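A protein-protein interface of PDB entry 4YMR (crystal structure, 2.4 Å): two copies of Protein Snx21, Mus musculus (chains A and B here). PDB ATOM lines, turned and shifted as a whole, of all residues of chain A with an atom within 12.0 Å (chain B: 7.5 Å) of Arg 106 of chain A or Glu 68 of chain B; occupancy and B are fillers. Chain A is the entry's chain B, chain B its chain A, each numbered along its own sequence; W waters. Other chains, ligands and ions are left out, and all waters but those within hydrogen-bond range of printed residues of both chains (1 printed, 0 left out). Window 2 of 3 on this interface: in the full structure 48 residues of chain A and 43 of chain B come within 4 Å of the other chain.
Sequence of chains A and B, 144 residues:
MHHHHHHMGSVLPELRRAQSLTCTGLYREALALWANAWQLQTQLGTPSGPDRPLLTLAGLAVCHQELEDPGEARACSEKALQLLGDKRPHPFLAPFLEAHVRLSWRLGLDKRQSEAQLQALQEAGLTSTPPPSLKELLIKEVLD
Water W1 lies within hydrogen-bond range of NE2 of Gln 65 of chain B (3.1 Å) and NH2 of Arg 102 of chain A (3.3 Å).
NH2 of Arg 102 of chain A lies close to NE2 of Gln 65 of chain B (3.4 Å).
OE2 of Glu 66 of chain B is in salt-bridge range of NZ of Lys 135 of chain A (2.7 Å).
OE1 of Glu 68 of chain B lies within salt-bridge range of NH2 of Arg 106 of chain A (2.4 Å).
No position is printed for both chains.
Of the 10 pairs that touch across the chains among the printed residues, none has its exchanged pair printed and touching as well.
Leu 103 of chain A touches Gln 65 of chain B.
Pro 70 of chain B touches Leu 103 of chain A.
Ala 73 of chain B touches Leu 103 of chain A.
CG of Pro 70 of chain B touches NH1 of Arg 106 of chain A (3.6 Å).
Pro 70 of chain B touches Leu 107 of chain A.
CA of Gly 71 of chain B touches CD1 of Leu 107 of chain A, 3.98 Å away.
Lys 135 of chain A touches Val 62 of chain B (CG to CG1, 3.5 Å).
NH1 of Arg 102 of chain A is in salt-bridge range of OE2 of Glu 98 of chain A.
Hydrophobic or aromatic side chains of chain A within 4 Å of the printed part of chain B: Leu 103 and Leu 107.
Among the printed residues, 10 pairs touch across the chains.
Among the printed residues, Asp or Glu carboxylates within 4 Å of a Lys or Arg side-chain nitrogen of the other chain: Arg 106 of chain A with Glu 68 of chain B and Lys 135 of chain A with Glu 66 of chain B.
Glu 98 of chain A touches none of the printed residues of chain B.
Of the printed residues of chain B, Leu 103 of chain A touches Gln 65, Pro 70 and Ala 73.
Arg 106 of chain A touches just these residues of chain B: Glu 68 (2.4 Å) and Pro 70 (3.6 Å).
Of the printed residues of chain B, Leu 107 of chain A touches Pro 70 and Gly 71.
His 64 of chain B touches none of the printed residues of chain A.
Printed residues of chain A within 4 Å of Glu 66 of chain B: Lys 135.
Of chain A, only Arg 106 comes within 4 Å of Glu 68 of chain B.
Of chain A, only Leu 103 (3.97 Å), Arg 106 (3.6 Å) and Leu 107 (3.96 Å) come within 4 Å of Pro 70 of chain B.
Printed residues of chain A within 4 Å of Gly 71 of chain B: Leu 107 (3.98 Å).
Of the printed residues of chain A, Ala 73 of chain B touches Leu 103 (3.7 Å).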
ATOM      1  N   LEU A  97      -0.176 -29.098  14.650  1.00  0.00           N
ATOM      2  CA  LEU A  97      -1.197 -28.214  15.205  1.00  0.00           C
ATOM      3  C   LEU A  97      -1.108 -26.826  14.585  1.00  0.00           C
ATOM      4  O   LEU A  97      -2.124 -26.183  14.349  1.00  0.00           O
ATOM      5  CB  LEU A  97      -1.088 -28.122  16.737  1.00  0.00           C
ATOM      6  CG  LEU A  97      -1.337 -29.408  17.540  1.00  0.00           C
ATOM      7  CD1 LEU A  97      -0.839 -29.270  18.973  1.00  0.00           C
ATOM      8  CD2 LEU A  97      -2.800 -29.793  17.515  1.00  0.00           C
ATOM      9  N   GLU A  98       0.104 -26.360  14.326  1.00  0.00           N
ATOM     10  CA  GLU A  98       0.264 -25.022  13.784  1.00  0.00           C
ATOM     11  C   GLU A  98      -0.371 -24.999  12.411  1.00  0.00           C
ATOM     12  O   GLU A  98      -1.159 -24.120  12.112  1.00  0.00           O
ATOM     13  CB  GLU A  98       1.737 -24.613  13.697  1.00  0.00           C
ATOM     14  CG  GLU A  98       1.930 -23.113  13.540  1.00  0.00           C
ATOM     15  CD  GLU A  98       1.825 -22.669  12.109  1.00  0.00           C
ATOM     16  OE1 GLU A  98       2.073 -23.520  11.224  1.00  0.00           O
ATOM     17  OE2 GLU A  98       1.486 -21.487  11.865  1.00  0.00           O
ATOM     18  N   ALA A  99      -0.015 -25.990  11.596  1.00  0.00           N
ATOM     19  CA  ALA A  99      -0.570 -26.171  10.275  1.00  0.00           C
ATOM     20  C   ALA A  99      -2.092 -26.262  10.333  1.00  0.00           C
ATOM     21  O   ALA A  99      -2.781 -25.661   9.526  1.00  0.00           O
ATOM     22  CB  ALA A  99       0.023 -27.428   9.613  1.00  0.00           C
ATOM     23  N   HIS A 100      -2.613 -26.999  11.303  1.00  0.00           N
ATOM     24  CA  HIS A 100      -4.051 -27.182  11.413  1.00  0.00           C
ATOM     25  C   HIS A 100      -4.783 -25.888  11.777  1.00  0.00           C
ATOM     26  O   HIS A 100      -5.851 -25.605  11.230  1.00  0.00           O
ATOM     27  CB  HIS A 100      -4.389 -28.306  12.401  1.00  0.00           C
ATOM     28  CG  HIS A 100      -5.852 -28.632  12.473  1.00  0.00           C
ATOM     29  ND1 HIS A 100      -6.666 -28.187  13.479  1.00  0.00           N
ATOM     30  CD2 HIS A 100      -6.641 -29.361  11.637  1.00  0.00           C
ATOM     31  CE1 HIS A 100      -7.904 -28.624  13.278  1.00  0.00           C
ATOM     32  NE2 HIS A 100      -7.907 -29.335  12.171  1.00  0.00           N
ATOM     33  N   VAL A 101      -4.201 -25.114  12.690  1.00  0.00           N
ATOM     34  CA  VAL A 101      -4.793 -23.855  13.122  1.00  0.00           C
ATOM     35  C   VAL A 101      -4.818 -22.881  11.961  1.00  0.00           C
ATOM     36  O   VAL A 101      -5.874 -22.378  11.599  1.00  0.00           O
ATOM     37  CB  VAL A 101      -4.034 -23.230  14.314  1.00  0.00           C
ATOM     38  CG1 VAL A 101      -4.462 -21.771  14.537  1.00  0.00           C
ATOM     39  CG2 VAL A 101      -4.252 -24.059  15.574  1.00  0.00           C
ATOM     40  N   ARG A 102      -3.648 -22.645  11.376  1.00  0.00           N
ATOM     41  CA  ARG A 102      -3.493 -21.765  10.224  1.00  0.00           C
ATOM     42  C   ARG A 102      -4.447 -22.106   9.079  1.00  0.00           C
ATOM     43  O   ARG A 102      -5.076 -21.224   8.508  1.00  0.00           O
ATOM     44  CB  ARG A 102      -2.044 -21.802   9.728  1.00  0.00           C
ATOM     45  CG  ARG A 102      -1.581 -20.527   9.044  1.00  0.00           C
ATOM     46  CD  ARG A 102      -0.121 -20.617   8.641  1.00  0.00           C
ATOM     47  NE  ARG A 102       0.094 -21.729   7.720  1.00  0.00           N
ATOM     48  CZ  ARG A 102       0.839 -22.792   7.992  1.00  0.00           C
ATOM     49  NH1 ARG A 102       1.457 -22.892   9.153  1.00  0.00           N
ATOM     50  NH2 ARG A 102       0.974 -23.752   7.098  1.00  0.00           N
ATOM     51  N   LEU A 103      -4.557 -23.386   8.748  1.00  0.00           N
ATOM     52  CA  LEU A 103      -5.356 -23.787   7.592  1.00  0.00           C
ATOM     53  C   LEU A 103      -6.861 -23.671   7.887  1.00  0.00           C
ATOM     54  O   LEU A 103      -7.639 -23.275   7.024  1.00  0.00           O
ATOM     55  CB  LEU A 103      -4.955 -25.188   7.094  1.00  0.00           C
ATOM     56  CG  LEU A 103      -3.538 -25.371   6.511  1.00  0.00           C
ATOM     57  CD1 LEU A 103      -3.129 -26.861   6.428  1.00  0.00           C
ATOM     58  CD2 LEU A 103      -3.406 -24.725   5.158  1.00  0.00           C
ATOM     59  N   SER A 104      -7.250 -24.005   9.114  1.00  0.00           N
ATOM     60  CA  SER A 104      -8.624 -23.888   9.578  1.00  0.00           C
ATOM     61  C   SER A 104      -9.128 -22.450   9.523  1.00  0.00           C
ATOM     62  O   SER A 104     -10.272 -22.190   9.139  1.00  0.00           O
ATOM     63  CB  SER A 104      -8.727 -24.396  11.013  1.00  0.00           C
ATOM     64  OG  SER A 104      -8.451 -25.776  11.103  1.00  0.00           O
ATOM     65  N   TRP A 105      -8.262 -21.525   9.918  1.00  0.00           N
ATOM     66  CA  TRP A 105      -8.572 -20.110   9.846  1.00  0.00           C
ATOM     67  C   TRP A 105      -8.738 -19.665   8.398  1.00  0.00           C
ATOM     68  O   TRP A 105      -9.764 -19.086   8.047  1.00  0.00           O
ATOM     69  CB  TRP A 105      -7.508 -19.266  10.564  1.00  0.00           C
ATOM     70  CG  TRP A 105      -7.794 -17.791  10.508  1.00  0.00           C
ATOM     71  CD1 TRP A 105      -7.169 -16.868   9.723  1.00  0.00           C
ATOM     72  CD2 TRP A 105      -8.797 -17.079  11.245  1.00  0.00           C
ATOM     73  NE1 TRP A 105      -7.706 -15.621   9.937  1.00  0.00           N
ATOM     74  CE2 TRP A 105      -8.709 -15.720  10.867  1.00  0.00           C
ATOM     75  CE3 TRP A 105      -9.758 -17.453  12.199  1.00  0.00           C
ATOM     76  CZ2 TRP A 105      -9.550 -14.731  11.402  1.00  0.00           C
ATOM     77  CZ3 TRP A 105     -10.591 -16.469  12.732  1.00  0.00           C
ATOM     78  CH2 TRP A 105     -10.481 -15.126  12.328  1.00  0.00           C
ATOM     79  N   ARG A 106      -7.733 -19.941   7.564  1.00  0.00           N
ATOM     80  CA  ARG A 106      -7.802 -19.673   6.117  1.00  0.00           C
ATOM     81  C   ARG A 106      -9.118 -20.177   5.515  1.00  0.00           C
ATOM     82  O   ARG A 106      -9.721 -19.518   4.688  1.00  0.00           O
ATOM     83  CB  ARG A 106      -6.635 -20.358   5.397  1.00  0.00           C
ATOM     84  CG  ARG A 106      -5.751 -19.464   4.491  1.00  0.00           C
ATOM     85  CD  ARG A 106      -4.578 -20.305   3.906  1.00  0.00           C
ATOM     86  NE  ARG A 106      -4.321 -20.167   2.462  1.00  0.00           N
ATOM     87  CZ  ARG A 106      -5.225 -20.305   1.485  1.00  0.00           C
ATOM     88  NH1 ARG A 106      -6.504 -20.564   1.739  1.00  0.00           N
ATOM     89  NH2 ARG A 106      -4.848 -20.168   0.230  1.00  0.00           N
ATOM     90  N   LEU A 107      -9.570 -21.347   5.944  1.00  0.00           N
ATOM     91  CA  LEU A 107     -10.698 -21.979   5.285  1.00  0.00           C
ATOM     92  C   LEU A 107     -12.013 -21.767   6.035  1.00  0.00           C
ATOM     93  O   LEU A 107     -13.030 -22.340   5.679  1.00  0.00           O
ATOM     94  CB  LEU A 107     -10.420 -23.471   5.085  1.00  0.00           C
ATOM     95  CG  LEU A 107      -9.269 -23.827   4.144  1.00  0.00           C
ATOM     96  CD1 LEU A 107      -8.959 -25.299   4.266  1.00  0.00           C
ATOM     97  CD2 LEU A 107      -9.627 -23.485   2.710  1.00  0.00           C
ATOM     98  N   GLY A 108     -11.983 -20.931   7.065  1.00  0.00           N
ATOM     99  CA  GLY A 108     -13.160 -20.657   7.864  1.00  0.00           C
ATOM    100  C   GLY A 108     -13.695 -21.849   8.637  1.00  0.00           C
ATOM    101  O   GLY A 108     -14.901 -21.990   8.804  1.00  0.00           O
ATOM    102  N   LEU A 109     -12.809 -22.721   9.106  1.00  0.00           N
ATOM    103  CA  LEU A 109     -13.244 -23.885   9.880  1.00  0.00           C
ATOM    104  C   LEU A 109     -12.760 -23.761  11.314  1.00  0.00           C
ATOM    105  O   LEU A 109     -11.952 -22.894  11.626  1.00  0.00           O
ATOM    106  CB  LEU A 109     -12.753 -25.197   9.262  1.00  0.00           C
ATOM    107  CG  LEU A 109     -13.501 -25.732   8.036  1.00  0.00           C
ATOM    108  CD1 LEU A 109     -12.949 -25.141   6.786  1.00  0.00           C
ATOM    109  CD2 LEU A 109     -13.389 -27.215   7.948  1.00  0.00           C
ATOM    110  N   ASP A 110     -13.260 -24.634  12.175  1.00  0.00           N
ATOM    111  CA  ASP A 110     -13.024 -24.521  13.609  1.00  0.00           C
ATOM    112  C   ASP A 110     -11.594 -24.909  14.017  1.00  0.00           C
ATOM    113  O   ASP A 110     -11.114 -25.996  13.678  1.00  0.00           O
ATOM    114  CB  ASP A 110     -14.038 -25.379  14.360  1.00  0.00           C
ATOM    115  CG  ASP A 110     -14.084 -25.068  15.840  1.00  0.00           C
ATOM    116  OD1 ASP A 110     -13.569 -24.011  16.238  1.00  0.00           O
ATOM    117  OD2 ASP A 110     -14.655 -25.874  16.600  1.00  0.00           O
ATOM    118  N   LYS A 111     -10.927 -24.015  14.749  1.00  0.00           N
ATOM    119  CA  LYS A 111      -9.560 -24.264  15.208  1.00  0.00           C
ATOM    120  C   LYS A 111      -9.450 -24.245  16.728  1.00  0.00           C
ATOM    121  O   LYS A 111      -8.366 -24.407  17.263  1.00  0.00           O
ATOM    122  CB  LYS A 111      -8.568 -23.245  14.607  1.00  0.00           C
ATOM    123  CG  LYS A 111      -9.041 -21.807  14.760  1.00  0.00           C
ATOM    124  CD  LYS A 111      -7.943 -20.746  14.737  1.00  0.00           C
ATOM    125  CE  LYS A 111      -8.363 -19.574  15.645  1.00  0.00           C
ATOM    126  NZ  LYS A 111      -7.422 -18.418  15.728  1.00  0.00           N
ATOM    127  N   ARG A 112     -10.562 -24.055  17.422  1.00  0.00           N
ATOM    128  CA  ARG A 112     -10.503 -23.865  18.873  1.00  0.00           C
ATOM    129  C   ARG A 112      -9.748 -24.958  19.630  1.00  0.00           C
ATOM    130  O   ARG A 112      -8.899 -24.666  20.482  1.00  0.00           O
ATOM    131  CB  ARG A 112     -11.901 -23.725  19.452  1.00  0.00           C
ATOM    132  CG  ARG A 112     -12.627 -22.489  19.004  1.00  0.00           C
ATOM    133  CD  ARG A 112     -14.066 -22.529  19.502  1.00  0.00           C
ATOM    134  NE  ARG A 112     -14.869 -23.503  18.767  1.00  0.00           N
ATOM    135  CZ  ARG A 112     -15.938 -24.128  19.254  1.00  0.00           C
ATOM    136  NH1 ARG A 112     -16.343 -23.894  20.494  1.00  0.00           N
ATOM    137  NH2 ARG A 112     -16.596 -24.994  18.498  1.00  0.00           N
ATOM    138  N   SER A 114      -7.599 -27.344  18.515  1.00  0.00           N
ATOM    139  CA  SER A 114      -6.235 -27.623  18.156  1.00  0.00           C
ATOM    140  C   SER A 114      -5.406 -26.442  18.629  1.00  0.00           C
ATOM    141  O   SER A 114      -4.320 -26.617  19.168  1.00  0.00           O
ATOM    142  CB  SER A 114      -6.102 -27.874  16.653  1.00  0.00           C
ATOM    143  OG  SER A 114      -6.318 -26.686  15.928  1.00  0.00           O
ATOM    144  N   GLU A 115      -5.940 -25.238  18.448  1.00  0.00           N
ATOM    145  CA  GLU A 115      -5.283 -24.039  18.968  1.00  0.00           C
ATOM    146  C   GLU A 115      -5.089 -24.034  20.485  1.00  0.00           C
ATOM    147  O   GLU A 115      -4.060 -23.564  20.970  1.00  0.00           O
ATOM    148  CB  GLU A 115      -6.004 -22.775  18.568  1.00  0.00           C
ATOM    149  CG  GLU A 115      -5.155 -21.568  18.854  1.00  0.00           C
ATOM    150  CD  GLU A 115      -5.719 -20.320  18.293  1.00  0.00           C
ATOM    151  OE1 GLU A 115      -6.908 -20.040  18.554  1.00  0.00           O
ATOM    152  OE2 GLU A 115      -4.968 -19.624  17.581  1.00  0.00           O
ATOM    153  N   LYS A 135       7.931 -27.827   7.127  1.00  0.00           N
ATOM    154  CA  LYS A 135       9.125 -27.755   6.283  1.00  0.00           C
ATOM    155  C   LYS A 135      10.460 -27.887   7.032  1.00  0.00           C
ATOM    156  O   LYS A 135      11.367 -28.572   6.560  1.00  0.00           O
ATOM    157  CB  LYS A 135       9.124 -26.456   5.472  1.00  0.00           C
ATOM    158  CG  LYS A 135       8.640 -26.623   4.057  1.00  0.00           C
ATOM    159  CD  LYS A 135       9.008 -25.443   3.151  1.00  0.00           C
ATOM    160  CE  LYS A 135       8.089 -24.248   3.375  1.00  0.00           C
ATOM    161  NZ  LYS A 135       8.234 -23.190   2.321  1.00  0.00           N
ATOM    162  N   ARG B  28       5.376 -30.011  -7.046  1.00  0.00           N
ATOM    163  CA  ARG B  28       4.509 -30.850  -7.867  1.00  0.00           C
ATOM    164  C   ARG B  28       5.135 -32.217  -8.176  1.00  0.00           C
ATOM    165  O   ARG B  28       4.441 -33.243  -8.129  1.00  0.00           O
ATOM    166  CB  ARG B  28       4.074 -30.117  -9.142  1.00  0.00           C
ATOM    167  CG  ARG B  28       2.954 -30.813  -9.904  1.00  0.00           C
ATOM    168  CD  ARG B  28       2.110 -29.817 -10.706  1.00  0.00           C
ATOM    169  NE  ARG B  28       1.208 -29.040  -9.857  1.00  0.00           N
ATOM    170  CZ  ARG B  28       0.089 -29.523  -9.327  1.00  0.00           C
ATOM    171  NH1 ARG B  28      -0.267 -30.775  -9.556  1.00  0.00           N
ATOM    172  NH2 ARG B  28      -0.674 -28.756  -8.565  1.00  0.00           N
ATOM    173  N   VAL B  62       2.929 -30.062   3.195  1.00  0.00           N
ATOM    174  CA  VAL B  62       3.792 -29.018   2.649  1.00  0.00           C
ATOM    175  C   VAL B  62       3.596 -28.797   1.160  1.00  0.00           C
ATOM    176  O   VAL B  62       3.440 -27.651   0.702  1.00  0.00           O
ATOM    177  CB  VAL B  62       5.284 -29.295   2.974  1.00  0.00           C
ATOM    178  CG1 VAL B  62       6.189 -28.367   2.197  1.00  0.00           C
ATOM    179  CG2 VAL B  62       5.513 -29.107   4.456  1.00  0.00           C
ATOM    180  N   CYS B  63       3.578 -29.900   0.414  1.00  0.00           N
ATOM    181  CA  CYS B  63       3.443 -29.826  -1.024  1.00  0.00           C
ATOM    182  C   CYS B  63       2.055 -29.319  -1.398  1.00  0.00           C
ATOM    183  O   CYS B  63       1.925 -28.452  -2.259  1.00  0.00           O
ATOM    184  CB  CYS B  63       3.760 -31.167  -1.701  1.00  0.00           C
ATOM    185  SG  CYS B  63       5.499 -31.632  -1.646  1.00  0.00           S
ATOM    186  N   HIS B  64       1.021 -29.841  -0.752  1.00  0.00           N
ATOM    187  CA  HIS B  64      -0.312 -29.314  -1.003  1.00  0.00           C
ATOM    188  C   HIS B  64      -0.390 -27.809  -0.707  1.00  0.00           C
ATOM    189  O   HIS B  64      -0.938 -27.065  -1.507  1.00  0.00           O
ATOM    190  CB  HIS B  64      -1.387 -30.133  -0.289  1.00  0.00           C
ATOM    191  CG  HIS B  64      -1.705 -31.421  -0.987  1.00  0.00           C
ATOM    192  ND1 HIS B  64      -1.879 -32.612  -0.309  1.00  0.00           N
ATOM    193  CD2 HIS B  64      -1.872 -31.705  -2.299  1.00  0.00           C
ATOM    194  CE1 HIS B  64      -2.151 -33.575  -1.182  1.00  0.00           C
ATOM    195  NE2 HIS B  64      -2.146 -33.049  -2.395  1.00  0.00           N
ATOM    196  N   GLN B  65       0.190 -27.349   0.399  1.00  0.00           N
ATOM    197  CA  GLN B  65       0.142 -25.916   0.711  1.00  0.00           C
ATOM    198  C   GLN B  65       0.846 -25.052  -0.312  1.00  0.00           C
ATOM    199  O   GLN B  65       0.378 -23.968  -0.645  1.00  0.00           O
ATOM    200  CB  GLN B  65       0.769 -25.641   2.062  1.00  0.00           C
ATOM    201  CG  GLN B  65      -0.156 -25.862   3.215  1.00  0.00           C
ATOM    202  CD  GLN B  65       0.509 -25.554   4.523  1.00  0.00           C
ATOM    203  OE1 GLN B  65       0.591 -24.394   4.932  1.00  0.00           O
ATOM    204  NE2 GLN B  65       1.012 -26.586   5.181  1.00  0.00           N
ATOM    205  N   GLU B  66       1.990 -25.534  -0.786  1.00  0.00           N
ATOM    206  CA  GLU B  66       2.756 -24.828  -1.803  1.00  0.00           C
ATOM    207  C   GLU B  66       2.050 -24.762  -3.159  1.00  0.00           C
ATOM    208  O   GLU B  66       2.401 -23.903  -3.992  1.00  0.00           O
ATOM    209  CB  GLU B  66       4.163 -25.426  -1.969  1.00  0.00           C
ATOM    210  CG  GLU B  66       5.017 -25.385  -0.682  1.00  0.00           C
ATOM    211  CD  GLU B  66       5.472 -23.978  -0.257  1.00  0.00           C
ATOM    212  OE1 GLU B  66       5.168 -22.989  -0.952  1.00  0.00           O
ATOM    213  OE2 GLU B  66       6.149 -23.858   0.788  1.00  0.00           O
ATOM    214  N   LEU B  67       1.023 -25.596  -3.353  1.00  0.00           N
ATOM    215  CA  LEU B  67       0.473 -25.844  -4.697  1.00  0.00           C
ATOM    216  C   LEU B  67      -0.907 -25.302  -5.210  1.00  0.00           C
ATOM    217  O   LEU B  67      -1.287 -25.648  -6.334  1.00  0.00           O
ATOM    218  CB  LEU B  67       0.505 -27.348  -4.999  1.00  0.00           C
ATOM    219  CG  LEU B  67       1.877 -27.917  -5.359  1.00  0.00           C
ATOM    220  CD1 LEU B  67       1.745 -29.429  -5.519  1.00  0.00           C
ATOM    221  CD2 LEU B  67       2.448 -27.261  -6.616  1.00  0.00           C
ATOM    222  N   GLU B  68      -1.702 -24.543  -4.469  1.00  0.00           N
ATOM    223  CA  GLU B  68      -1.861 -24.648  -3.070  1.00  0.00           C
ATOM    224  C   GLU B  68      -3.252 -25.300  -2.989  1.00  0.00           C
ATOM    225  O   GLU B  68      -4.252 -24.737  -3.449  1.00  0.00           O
ATOM    226  CB  GLU B  68      -1.892 -23.275  -2.451  1.00  0.00           C
ATOM    227  CG  GLU B  68      -2.749 -22.256  -3.196  1.00  0.00           C
ATOM    228  CD  GLU B  68      -3.172 -21.163  -2.261  1.00  0.00           C
ATOM    229  OE1 GLU B  68      -4.384 -21.065  -1.948  1.00  0.00           O
ATOM    230  OE2 GLU B  68      -2.277 -20.395  -1.846  1.00  0.00           O
ATOM    231  N   ASP B  69      -3.301 -26.535  -2.511  1.00  0.00           N
ATOM    232  CA  ASP B  69      -4.547 -27.131  -2.142  1.00  0.00           C
ATOM    233  C   ASP B  69      -4.532 -27.032  -0.587  1.00  0.00           C
ATOM    234  O   ASP B  69      -4.062 -27.950   0.102  1.00  0.00           O
ATOM    235  CB  ASP B  69      -4.589 -28.584  -2.680  1.00  0.00           C
ATOM    236  CG  ASP B  69      -3.964 -28.723  -4.107  1.00  0.00           C
ATOM    237  OD1 ASP B  69      -4.336 -27.939  -5.002  1.00  0.00           O
ATOM    238  OD2 ASP B  69      -3.083 -29.593  -4.331  1.00  0.00           O
ATOM    239  N   PRO B  70      -4.993 -25.892  -0.030  1.00  0.00           N
ATOM    240  CA  PRO B  70      -4.986 -25.829   1.431  1.00  0.00           C
ATOM    241  C   PRO B  70      -5.965 -26.841   2.050  1.00  0.00           C
ATOM    242  O   PRO B  70      -5.722 -27.301   3.168  1.00  0.00           O
ATOM    243  CB  PRO B  70      -5.379 -24.368   1.728  1.00  0.00           C
ATOM    244  CG  PRO B  70      -6.121 -23.925   0.538  1.00  0.00           C
ATOM    245  CD  PRO B  70      -5.463 -24.620  -0.626  1.00  0.00           C
ATOM    246  N   GLY B  71      -7.031 -27.187   1.325  1.00  0.00           N
ATOM    247  CA  GLY B  71      -7.965 -28.213   1.750  1.00  0.00           C
ATOM    248  C   GLY B  71      -7.273 -29.551   1.920  1.00  0.00           C
ATOM    249  O   GLY B  71      -7.365 -30.164   2.986  1.00  0.00           O
ATOM    250  N   GLU B  72      -6.571 -29.996   0.874  1.00  0.00           N
ATOM    251  CA  GLU B  72      -5.791 -31.246   0.926  1.00  0.00           C
ATOM    252  C   GLU B  72      -4.696 -31.227   1.993  1.00  0.00           C
ATOM    253  O   GLU B  72      -4.414 -32.253   2.605  1.00  0.00           O
ATOM    254  CB  GLU B  72      -5.201 -31.613  -0.445  1.00  0.00           C
ATOM    255  CG  GLU B  72      -6.226 -32.114  -1.446  1.00  0.00           C
ATOM    256  CD  GLU B  72      -6.980 -33.332  -0.943  1.00  0.00           C
ATOM    257  OE1 GLU B  72      -6.335 -34.344  -0.583  1.00  0.00           O
ATOM    258  OE2 GLU B  72      -8.226 -33.267  -0.899  1.00  0.00           O
ATOM    259  N   ALA B  73      -4.090 -30.061   2.212  1.00  0.00           N
ATOM    260  CA  ALA B  73      -3.104 -29.906   3.278  1.00  0.00           C
ATOM    261  C   ALA B  73      -3.762 -30.044   4.638  1.00  0.00           C
ATOM    262  O   ALA B  73      -3.199 -30.638   5.543  1.00  0.00           O
ATOM    263  CB  ALA B  73      -2.372 -28.563   3.163  1.00  0.00           C
HETATM  264  O   HOH W   1       3.410 -25.971   7.096  1.00  0.00           O
